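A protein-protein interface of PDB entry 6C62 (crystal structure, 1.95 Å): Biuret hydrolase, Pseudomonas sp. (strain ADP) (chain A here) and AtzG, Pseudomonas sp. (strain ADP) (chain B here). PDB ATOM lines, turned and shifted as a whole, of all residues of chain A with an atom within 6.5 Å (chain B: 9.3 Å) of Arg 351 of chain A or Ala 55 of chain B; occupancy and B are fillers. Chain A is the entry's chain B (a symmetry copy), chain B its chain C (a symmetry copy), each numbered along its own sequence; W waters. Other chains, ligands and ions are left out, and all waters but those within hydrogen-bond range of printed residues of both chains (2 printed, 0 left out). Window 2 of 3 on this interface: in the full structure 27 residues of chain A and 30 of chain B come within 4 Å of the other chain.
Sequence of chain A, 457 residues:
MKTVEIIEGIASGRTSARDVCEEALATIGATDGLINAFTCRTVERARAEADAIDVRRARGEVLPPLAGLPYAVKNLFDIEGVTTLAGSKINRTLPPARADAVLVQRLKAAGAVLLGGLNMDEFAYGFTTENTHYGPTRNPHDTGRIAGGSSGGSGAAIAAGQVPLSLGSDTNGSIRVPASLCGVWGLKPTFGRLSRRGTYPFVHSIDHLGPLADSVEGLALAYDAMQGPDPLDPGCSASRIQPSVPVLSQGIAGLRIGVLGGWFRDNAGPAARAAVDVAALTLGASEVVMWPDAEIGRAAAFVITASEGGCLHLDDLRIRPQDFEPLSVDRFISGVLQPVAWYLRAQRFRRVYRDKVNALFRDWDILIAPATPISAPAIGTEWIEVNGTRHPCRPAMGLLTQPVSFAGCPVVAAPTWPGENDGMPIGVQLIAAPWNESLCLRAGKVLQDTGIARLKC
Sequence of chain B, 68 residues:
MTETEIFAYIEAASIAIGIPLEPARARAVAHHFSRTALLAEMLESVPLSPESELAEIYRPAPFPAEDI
The guanidinium group (NH1) of Arg 354 of chain A is in salt-bridge range of the side-chain carboxylate (OE2) of Glu 56 of chain B (2.8 Å). The guanidinium group (NH2) of Arg 351 of chain A lies within hydrogen-bond range of the backbone carbonyl oxygen (O) of Ala 55 of chain B (3.1 Å). The guanidinium group (NE) of Arg 351 of chain A lies within hydrogen-bond range of the backbone carbonyl oxygen (O) of Glu 53 of chain B, 3.4 Å away. The guanidinium group (NE) of Arg 351 of chain A lies within hydrogen-bond range of the backbone carbonyl oxygen (O) of Leu 54 of chain B (2.9 Å). The backbone carbonyl oxygen (O) of Ala 55 of chain B lies within hydrogen-bond range of the guanidinium group (NH2) of Arg 354 of chain A (3.0 Å). The guanidinium group (NH2) of Arg 348 of chain A sits at hydrogen-bond distance from the backbone carbonyl oxygen (O) of Ser 49 of chain B (2.8 Å). The backbone NH (N) of Ala 55 of chain B sits at hydrogen-bond distance from the backbone carbonyl oxygen (O) of Gln 347 of chain A (3.1 Å). The guanidinium group of Arg 348 of chain A lies within hydrogen-bond range of the backbone carbonyl oxygen of Ser 52 of chain B, 3.0 Å away.
OG of Ser 52 of chain B lies within hydrogen-bond range of N of Ser 49 of chain B (2.9 Å). OE1 of Glu 56 of chain B is in salt-bridge range of NH1 of Arg 59 of chain B (3.2 Å).
CB of Ala 346 of chain A touches CD2 of Leu 43 of chain B, 3.6 Å away. CD2 of Leu 54 of chain B touches CB of Gln 347 of chain A, 3.8 Å away. CB of Leu 48 of chain B touches NH2 of Arg 348 of chain A (3.8 Å). Glu 53 of chain B touches Arg 348 of chain A (O to CA, 3.7 Å). CG of Arg 348 of chain A touches CD2 of Leu 54 of chain B, 3.9 Å away. CB of Phe 349 of chain A touches CD1 of Leu 43 of chain B, at 3.8 Å. Val 46 of chain B touches Phe 349 of chain A. Arg 350 of chain A touches Ala 55 of chain B (CB to CB, 3.97 Å). Val 352 of chain A touches Leu 48 of chain B.
Asp 355 of chain A touches none of the printed residues of chain B. Of the printed residues of chain A, Leu 43 of chain B touches Ala 346 (3.6 Å) and Phe 349 (3.8 Å). Printed residues of chain A within 4 Å of Glu 53 of chain B: Arg 348 and Arg 351. Of the printed residues of chain A, Leu 54 of chain B touches Gln 347, Arg 348 and Arg 351. Of the printed residues of chain A, Ala 55 of chain B touches Gln 347, Arg 350, Arg 351 and Arg 354. Tyr 58 of chain B touches none of the printed residues of chain A. The nearest residue of chain B that does not touch Arg 351 of chain A is Ile 57 of chain B (4.2 Å). The nearest printed residue of chain A that does not touch Glu 53 of chain B is Gln 347 of chain A (4.5 Å).
Of the 11 printed residues of chain A, 8 touch a printed residue of chain B. Hydrophobic or aromatic side chains of chain A within 4 Å of the printed part of chain B: Ala 346, Phe 349 and Val 352. Printed residues of chain B that touch a printed residue of chain A: Leu 43, Val 46, Leu 48, Ser 49, Ser 52, Glu 53, Leu 54, Ala 55 and Glu 56. Among the printed residues, 17 pairs touch across the chains. Among the printed residues, Asp or Glu carboxylates within 4 Å of a Lys or Arg side-chain nitrogen of the other chain: Arg 354 of chain A with Glu 56 of chain B (2.8 Å).
Water W2 bridges O of Glu 53 of chain B (2.6 Å) and O of Arg 348 of chain A (2.7 Å). Water W1 lies within hydrogen-bond range of the backbone NH (N) of Glu 56 of chain B (3.0 Å), the side-chain amide oxygen (OE1) of Gln 347 of chain A (3.1 Å) and the backbone NH (N) of Ala 55 of chain B (3.2 Å).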
ATOM      1  N   ALA A 346       9.049  -2.740  14.226  1.00  0.00           N
ATOM      2  CA  ALA A 346       8.909  -3.140  12.844  1.00  0.00           C
ATOM      3  C   ALA A 346       8.400  -2.046  11.912  1.00  0.00           C
ATOM      4  O   ALA A 346       8.918  -1.882  10.785  1.00  0.00           O
ATOM      5  CB  ALA A 346       8.033  -4.380  12.766  1.00  0.00           C
ATOM      6  N   GLN A 347       7.463  -1.256  12.370  1.00  0.00           N
ATOM      7  CA  GLN A 347       6.954  -0.117  11.607  1.00  0.00           C
ATOM      8  C   GLN A 347       8.018   1.008  11.451  1.00  0.00           C
ATOM      9  O   GLN A 347       8.070   1.680  10.377  1.00  0.00           O
ATOM     10  CB  GLN A 347       5.681   0.433  12.206  1.00  0.00           C
ATOM     11  CG  GLN A 347       4.415  -0.423  12.033  1.00  0.00           C
ATOM     12  CD  GLN A 347       3.898  -0.471  10.581  1.00  0.00           C
ATOM     13  OE1 GLN A 347       4.534   0.066   9.672  1.00  0.00           O
ATOM     14  NE2 GLN A 347       2.740  -1.174  10.343  1.00  0.00           N
ATOM     15  N   ARG A 348       8.865   1.188  12.466  1.00  0.00           N
ATOM     16  CA  ARG A 348       9.920   2.167  12.398  1.00  0.00           C
ATOM     17  C   ARG A 348      11.030   1.663  11.487  1.00  0.00           C
ATOM     18  O   ARG A 348      11.572   2.427  10.671  1.00  0.00           O
ATOM     19  CB  ARG A 348      10.467   2.518  13.788  1.00  0.00           C
ATOM     20  CG  ARG A 348       9.429   3.291  14.588  1.00  0.00           C
ATOM     21  CD  ARG A 348       9.777   3.447  16.081  1.00  0.00           C
ATOM     22  NE  ARG A 348      10.953   4.264  16.263  1.00  0.00           N
ATOM     23  CZ  ARG A 348      11.823   4.159  17.266  1.00  0.00           C
ATOM     24  NH1 ARG A 348      11.680   3.283  18.235  1.00  0.00           N
ATOM     25  NH2 ARG A 348      12.884   4.944  17.283  1.00  0.00           N
ATOM     26  N   PHE A 349      11.357   0.377  11.608  1.00  0.00           N
ATOM     27  CA  PHE A 349      12.325  -0.234  10.721  1.00  0.00           C
ATOM     28  C   PHE A 349      11.847  -0.166   9.268  1.00  0.00           C
ATOM     29  O   PHE A 349      12.639   0.028   8.356  1.00  0.00           O
ATOM     30  CB  PHE A 349      12.593  -1.677  11.120  1.00  0.00           C
ATOM     31  CG  PHE A 349      13.405  -2.425  10.091  1.00  0.00           C
ATOM     32  CD1 PHE A 349      14.765  -2.157   9.937  1.00  0.00           C
ATOM     33  CD2 PHE A 349      12.827  -3.325   9.293  1.00  0.00           C
ATOM     34  CE1 PHE A 349      15.512  -2.806   8.947  1.00  0.00           C
ATOM     35  CE2 PHE A 349      13.548  -3.943   8.278  1.00  0.00           C
ATOM     36  CZ  PHE A 349      14.872  -3.700   8.126  1.00  0.00           C
ATOM     37  N   ARG A 350      10.535  -0.306   9.031  1.00  0.00           N
ATOM     38  CA  ARG A 350      10.044  -0.275   7.668  1.00  0.00           C
ATOM     39  C   ARG A 350      10.374   1.035   6.925  1.00  0.00           C
ATOM     40  O   ARG A 350      10.582   1.000   5.716  1.00  0.00           O
ATOM     41  CB  ARG A 350       8.506  -0.528   7.621  1.00  0.00           C
ATOM     42  CG  ARG A 350       8.005  -0.863   6.235  1.00  0.00           C
ATOM     43  CD  ARG A 350       6.523  -1.183   6.234  1.00  0.00           C
ATOM     44  NE  ARG A 350       6.158  -1.958   5.049  1.00  0.00           N
ATOM     45  CZ  ARG A 350       4.887  -2.281   4.743  1.00  0.00           C
ATOM     46  NH1 ARG A 350       3.899  -1.900   5.518  1.00  0.00           N
ATOM     47  NH2 ARG A 350       4.632  -3.017   3.657  1.00  0.00           N
ATOM     48  N   ARG A 351      10.398   2.172   7.620  1.00  0.00           N
ATOM     49  CA  ARG A 351      10.874   3.457   7.011  1.00  0.00           C
ATOM     50  C   ARG A 351      12.338   3.341   6.568  1.00  0.00           C
ATOM     51  O   ARG A 351      12.678   3.708   5.441  1.00  0.00           O
ATOM     52  CB  ARG A 351      10.671   4.623   7.944  1.00  0.00           C
ATOM     53  CG  ARG A 351      11.381   5.919   7.512  1.00  0.00           C
ATOM     54  CD  ARG A 351      11.017   7.143   8.354  1.00  0.00           C
ATOM     55  NE  ARG A 351       9.571   7.396   8.296  1.00  0.00           N
ATOM     56  CZ  ARG A 351       8.956   8.090   7.332  1.00  0.00           C
ATOM     57  NH1 ARG A 351       9.609   8.650   6.367  1.00  0.00           N
ATOM     58  NH2 ARG A 351       7.648   8.247   7.379  1.00  0.00           N
ATOM     59  N   VAL A 352      13.196   2.805   7.437  1.00  0.00           N
ATOM     60  CA  VAL A 352      14.620   2.645   7.127  1.00  0.00           C
ATOM     61  C   VAL A 352      14.758   1.714   5.894  1.00  0.00           C
ATOM     62  O   VAL A 352      15.482   1.997   4.960  1.00  0.00           O
ATOM     63  CB  VAL A 352      15.401   2.042   8.322  1.00  0.00           C
ATOM     64  CG1 VAL A 352      16.835   1.677   7.895  1.00  0.00           C
ATOM     65  CG2 VAL A 352      15.431   3.029   9.472  1.00  0.00           C
ATOM     66  N   TYR A 353      14.025   0.620   5.937  1.00  0.00           N
ATOM     67  CA  TYR A 353      14.041  -0.397   4.888  1.00  0.00           C
ATOM     68  C   TYR A 353      13.590   0.180   3.545  1.00  0.00           C
ATOM     69  O   TYR A 353      14.254  -0.090   2.529  1.00  0.00           O
ATOM     70  CB  TYR A 353      13.164  -1.543   5.320  1.00  0.00           C
ATOM     71  CG  TYR A 353      13.227  -2.795   4.510  1.00  0.00           C
ATOM     72  CD1 TYR A 353      14.310  -3.612   4.590  1.00  0.00           C
ATOM     73  CD2 TYR A 353      12.118  -3.221   3.761  1.00  0.00           C
ATOM     74  CE1 TYR A 353      14.356  -4.806   3.910  1.00  0.00           C
ATOM     75  CE2 TYR A 353      12.142  -4.421   3.103  1.00  0.00           C
ATOM     76  CZ  TYR A 353      13.273  -5.214   3.168  1.00  0.00           C
ATOM     77  OH  TYR A 353      13.351  -6.414   2.552  1.00  0.00           O
ATOM     78  N   ARG A 354      12.461   0.902   3.545  1.00  0.00           N
ATOM     79  CA  ARG A 354      11.946   1.571   2.341  1.00  0.00           C
ATOM     80  C   ARG A 354      13.043   2.462   1.721  1.00  0.00           C
ATOM     81  O   ARG A 354      13.316   2.370   0.525  1.00  0.00           O
ATOM     82  CB  ARG A 354      10.710   2.422   2.628  1.00  0.00           C
ATOM     83  CG  ARG A 354      10.174   3.244   1.460  1.00  0.00           C
ATOM     84  CD  ARG A 354       8.798   3.824   1.794  1.00  0.00           C
ATOM     85  NE  ARG A 354       8.888   4.731   2.915  1.00  0.00           N
ATOM     86  CZ  ARG A 354       7.888   5.071   3.712  1.00  0.00           C
ATOM     87  NH1 ARG A 354       6.660   4.607   3.563  1.00  0.00           N
ATOM     88  NH2 ARG A 354       8.102   5.925   4.684  1.00  0.00           N
ATOM     89  N   ASP A 355      13.699   3.260   2.566  1.00  0.00           N
ATOM     90  CA  ASP A 355      14.762   4.132   2.103  1.00  0.00           C
ATOM     91  C   ASP A 355      15.875   3.337   1.465  1.00  0.00           C
ATOM     92  O   ASP A 355      16.369   3.751   0.393  1.00  0.00           O
ATOM     93  CB  ASP A 355      15.294   5.092   3.205  1.00  0.00           C
ATOM     94  CG  ASP A 355      14.269   6.159   3.629  1.00  0.00           C
ATOM     95  OD1 ASP A 355      13.311   6.478   2.848  1.00  0.00           O
ATOM     96  OD2 ASP A 355      14.397   6.747   4.736  1.00  0.00           O
ATOM     97  N   LYS A 356      16.297   2.238   2.083  1.00  0.00           N
ATOM     98  CA  LYS A 356      17.402   1.449   1.581  1.00  0.00           C
ATOM     99  C   LYS A 356      17.064   0.723   0.250  1.00  0.00           C
ATOM    100  O   LYS A 356      17.900   0.615  -0.656  1.00  0.00           O
ATOM    101  CB  LYS A 356      17.856   0.420   2.615  1.00  0.00           C
ATOM    102  CG  LYS A 356      18.619   1.051   3.767  1.00  0.00           C
ATOM    103  CD  LYS A 356      19.064  -0.026   4.735  1.00  0.00           C
ATOM    104  CE  LYS A 356      19.884   0.563   5.846  1.00  0.00           C
ATOM    105  NZ  LYS A 356      20.482  -0.579   6.546  1.00  0.00           N
ATOM    106  N   LEU B  43      15.306  -7.876  15.145  1.00  0.00           N
ATOM    107  CA  LEU B  43      14.854  -6.522  14.834  1.00  0.00           C
ATOM    108  C   LEU B  43      15.414  -5.501  15.836  1.00  0.00           C
ATOM    109  O   LEU B  43      15.699  -4.364  15.469  1.00  0.00           O
ATOM    110  CB  LEU B  43      13.326  -6.509  14.821  1.00  0.00           C
ATOM    111  CG  LEU B  43      12.544  -5.353  14.246  1.00  0.00           C
ATOM    112  CD1 LEU B  43      13.078  -4.974  12.887  1.00  0.00           C
ATOM    113  CD2 LEU B  43      11.084  -5.768  14.197  1.00  0.00           C
ATOM    114  N   VAL B  46      18.755  -3.589  15.070  1.00  0.00           N
ATOM    115  CA  VAL B  46      18.820  -2.429  14.170  1.00  0.00           C
ATOM    116  C   VAL B  46      18.918  -1.109  14.938  1.00  0.00           C
ATOM    117  O   VAL B  46      18.106  -0.857  15.821  1.00  0.00           O
ATOM    118  CB  VAL B  46      17.582  -2.382  13.254  1.00  0.00           C
ATOM    119  CG1 VAL B  46      17.475  -1.061  12.482  1.00  0.00           C
ATOM    120  CG2 VAL B  46      17.657  -3.519  12.262  1.00  0.00           C
ATOM    121  N   LEU B  48      18.052   2.387  15.749  1.00  0.00           N
ATOM    122  CA  LEU B  48      17.062   3.384  15.465  1.00  0.00           C
ATOM    123  C   LEU B  48      17.347   4.479  16.466  1.00  0.00           C
ATOM    124  O   LEU B  48      17.782   4.213  17.603  1.00  0.00           O
ATOM    125  CB  LEU B  48      15.674   2.816  15.717  1.00  0.00           C
ATOM    126  CG  LEU B  48      15.235   1.710  14.758  1.00  0.00           C
ATOM    127  CD1 LEU B  48      13.895   1.182  15.201  1.00  0.00           C
ATOM    128  CD2 LEU B  48      15.159   2.216  13.339  1.00  0.00           C
ATOM    129  N   SER B  49      17.135   5.693  16.071  1.00  0.00           N
ATOM    130  CA  SER B  49      17.220   6.821  16.981  1.00  0.00           C
ATOM    131  C   SER B  49      15.775   7.239  17.323  1.00  0.00           C
ATOM    132  O   SER B  49      14.816   6.861  16.618  1.00  0.00           O
ATOM    133  CB  SER B  49      17.883   7.997  16.259  1.00  0.00           C
ATOM    134  OG  SER B  49      19.124   7.704  15.665  1.00  0.00           O
ATOM    135  N   GLU B  51      14.336   9.916  16.639  1.00  0.00           N
ATOM    136  CA  GLU B  51      13.764  10.586  15.492  1.00  0.00           C
ATOM    137  C   GLU B  51      13.627   9.655  14.265  1.00  0.00           C
ATOM    138  O   GLU B  51      13.273  10.139  13.212  1.00  0.00           O
ATOM    139  CB  GLU B  51      14.587  11.841  15.144  1.00  0.00           C
ATOM    140  CG  GLU B  51      16.011  11.555  14.699  1.00  0.00           C
ATOM    141  CD  GLU B  51      17.114  11.630  15.820  1.00  0.00           C
ATOM    142  OE1 GLU B  51      16.869  11.497  17.092  1.00  0.00           O
ATOM    143  OE2 GLU B  51      18.299  11.785  15.395  1.00  0.00           O
ATOM    144  N   SER B  52      13.949   8.360  14.374  1.00  0.00           N
ATOM    145  CA  SER B  52      13.560   7.399  13.334  1.00  0.00           C
ATOM    146  C   SER B  52      12.075   7.153  13.475  1.00  0.00           C
ATOM    147  O   SER B  52      11.638   6.450  14.391  1.00  0.00           O
ATOM    148  CB  SER B  52      14.287   6.060  13.488  1.00  0.00           C
ATOM    149  OG  SER B  52      15.680   6.282  13.648  1.00  0.00           O
ATOM    150  N   GLU B  53      11.308   7.736  12.595  1.00  0.00           N
ATOM    151  CA  GLU B  53       9.872   7.665  12.681  1.00  0.00           C
ATOM    152  C   GLU B  53       9.212   6.427  12.058  1.00  0.00           C
ATOM    153  O   GLU B  53       9.768   5.733  11.267  1.00  0.00           O
ATOM    154  CB  GLU B  53       9.251   8.962  12.086  1.00  0.00           C
ATOM    155  CG  GLU B  53       9.796  10.224  12.794  1.00  0.00           C
ATOM    156  CD  GLU B  53       8.981  11.473  12.550  1.00  0.00           C
ATOM    157  OE1 GLU B  53       7.754  11.370  12.383  1.00  0.00           O
ATOM    158  OE2 GLU B  53       9.568  12.571  12.532  1.00  0.00           O
ATOM    159  N   LEU B  54       7.967   6.232  12.414  1.00  0.00           N
ATOM    160  CA  LEU B  54       7.078   5.276  11.749  1.00  0.00           C
ATOM    161  C   LEU B  54       7.067   5.529  10.227  1.00  0.00           C
ATOM    162  O   LEU B  54       7.179   6.657   9.778  1.00  0.00           O
ATOM    163  CB  LEU B  54       5.662   5.412  12.296  1.00  0.00           C
ATOM    164  CG  LEU B  54       5.433   5.165  13.803  1.00  0.00           C
ATOM    165  CD1 LEU B  54       4.088   5.715  14.246  1.00  0.00           C
ATOM    166  CD2 LEU B  54       5.559   3.687  14.231  1.00  0.00           C
ATOM    167  N   ALA B  55       6.927   4.444   9.477  1.00  0.00           N
ATOM    168  CA  ALA B  55       6.825   4.474   8.048  1.00  0.00           C
ATOM    169  C   ALA B  55       5.651   5.327   7.570  1.00  0.00           C
ATOM    170  O   ALA B  55       5.780   5.983   6.545  1.00  0.00           O
ATOM    171  CB  ALA B  55       6.755   3.037   7.486  1.00  0.00           C
ATOM    172  N   GLU B  56       4.550   5.389   8.319  1.00  0.00           N
ATOM    173  CA  GLU B  56       3.437   6.264   7.938  1.00  0.00           C
ATOM    174  C   GLU B  56       2.953   7.127   9.093  1.00  0.00           C
ATOM    175  O   GLU B  56       2.628   6.640  10.206  1.00  0.00           O
ATOM    176  CB  GLU B  56       2.269   5.433   7.351  1.00  0.00           C
ATOM    177  CG  GLU B  56       2.647   4.730   6.049  1.00  0.00           C
ATOM    178  CD  GLU B  56       3.113   5.684   4.910  1.00  0.00           C
ATOM    179  OE1 GLU B  56       2.642   6.804   4.828  1.00  0.00           O
ATOM    180  OE2 GLU B  56       3.995   5.363   4.097  1.00  0.00           O
ATOM    181  N   ILE B  57       2.884   8.410   8.821  1.00  0.00           N
ATOM    182  CA  ILE B  57       2.499   9.371   9.824  1.00  0.00           C
ATOM    183  C   ILE B  57       1.117   9.936   9.417  1.00  0.00           C
ATOM    184  O   ILE B  57       0.870  10.205   8.248  1.00  0.00           O
ATOM    185  CB  ILE B  57       3.570  10.504   9.910  1.00  0.00           C
ATOM    186  CG1 ILE B  57       4.977   9.952  10.199  1.00  0.00           C
ATOM    187  CG2 ILE B  57       3.163  11.554  10.933  1.00  0.00           C
ATOM    188  CD1 ILE B  57       5.018   9.185  11.528  1.00  0.00           C
ATOM    189  N   TYR B  58       0.257  10.125  10.404  1.00  0.00           N
ATOM    190  CA  TYR B  58      -1.081  10.686  10.258  1.00  0.00           C
ATOM    191  C   TYR B  58      -1.223  11.913   9.368  1.00  0.00           C
ATOM    192  O   TYR B  58      -0.405  12.805   9.389  1.00  0.00           O
ATOM    193  CB  TYR B  58      -1.621  10.980  11.617  1.00  0.00           C
ATOM    194  CG  TYR B  58      -3.070  11.377  11.670  1.00  0.00           C
ATOM    195  CD1 TYR B  58      -4.053  10.452  11.421  1.00  0.00           C
ATOM    196  CD2 TYR B  58      -3.444  12.623  12.058  1.00  0.00           C
ATOM    197  CE1 TYR B  58      -5.368  10.764  11.514  1.00  0.00           C
ATOM    198  CE2 TYR B  58      -4.791  12.966  12.150  1.00  0.00           C
ATOM    199  CZ  TYR B  58      -5.729  12.037  11.910  1.00  0.00           C
ATOM    200  OH  TYR B  58      -7.030  12.393  11.941  1.00  0.00           O
ATOM    201  N   ARG B  59      -2.267  11.909   8.556  1.00  0.00           N
ATOM    202  CA  ARG B  59      -2.643  13.040   7.699  1.00  0.00           C
ATOM    203  C   ARG B  59      -4.079  13.365   8.119  1.00  0.00           C
ATOM    204  O   ARG B  59      -4.970  12.537   7.976  1.00  0.00           O
ATOM    205  CB  ARG B  59      -2.560  12.648   6.239  1.00  0.00           C
ATOM    206  CG  ARG B  59      -1.152  12.195   5.790  1.00  0.00           C
ATOM    207  CD  ARG B  59      -1.261  11.389   4.535  1.00  0.00           C
ATOM    208  NE  ARG B  59       0.035  11.024   3.951  1.00  0.00           N
ATOM    209  CZ  ARG B  59       0.717   9.902   4.192  1.00  0.00           C
ATOM    210  NH1 ARG B  59       0.284   8.978   5.052  1.00  0.00           N
ATOM    211  NH2 ARG B  59       1.880   9.706   3.563  1.00  0.00           N
HETATM  212  O   HOH W   1       4.098   3.099  10.166  1.00  0.00           O
HETATM  213  O   HOH W   2      12.269   5.012  11.110  1.00  0.00           O
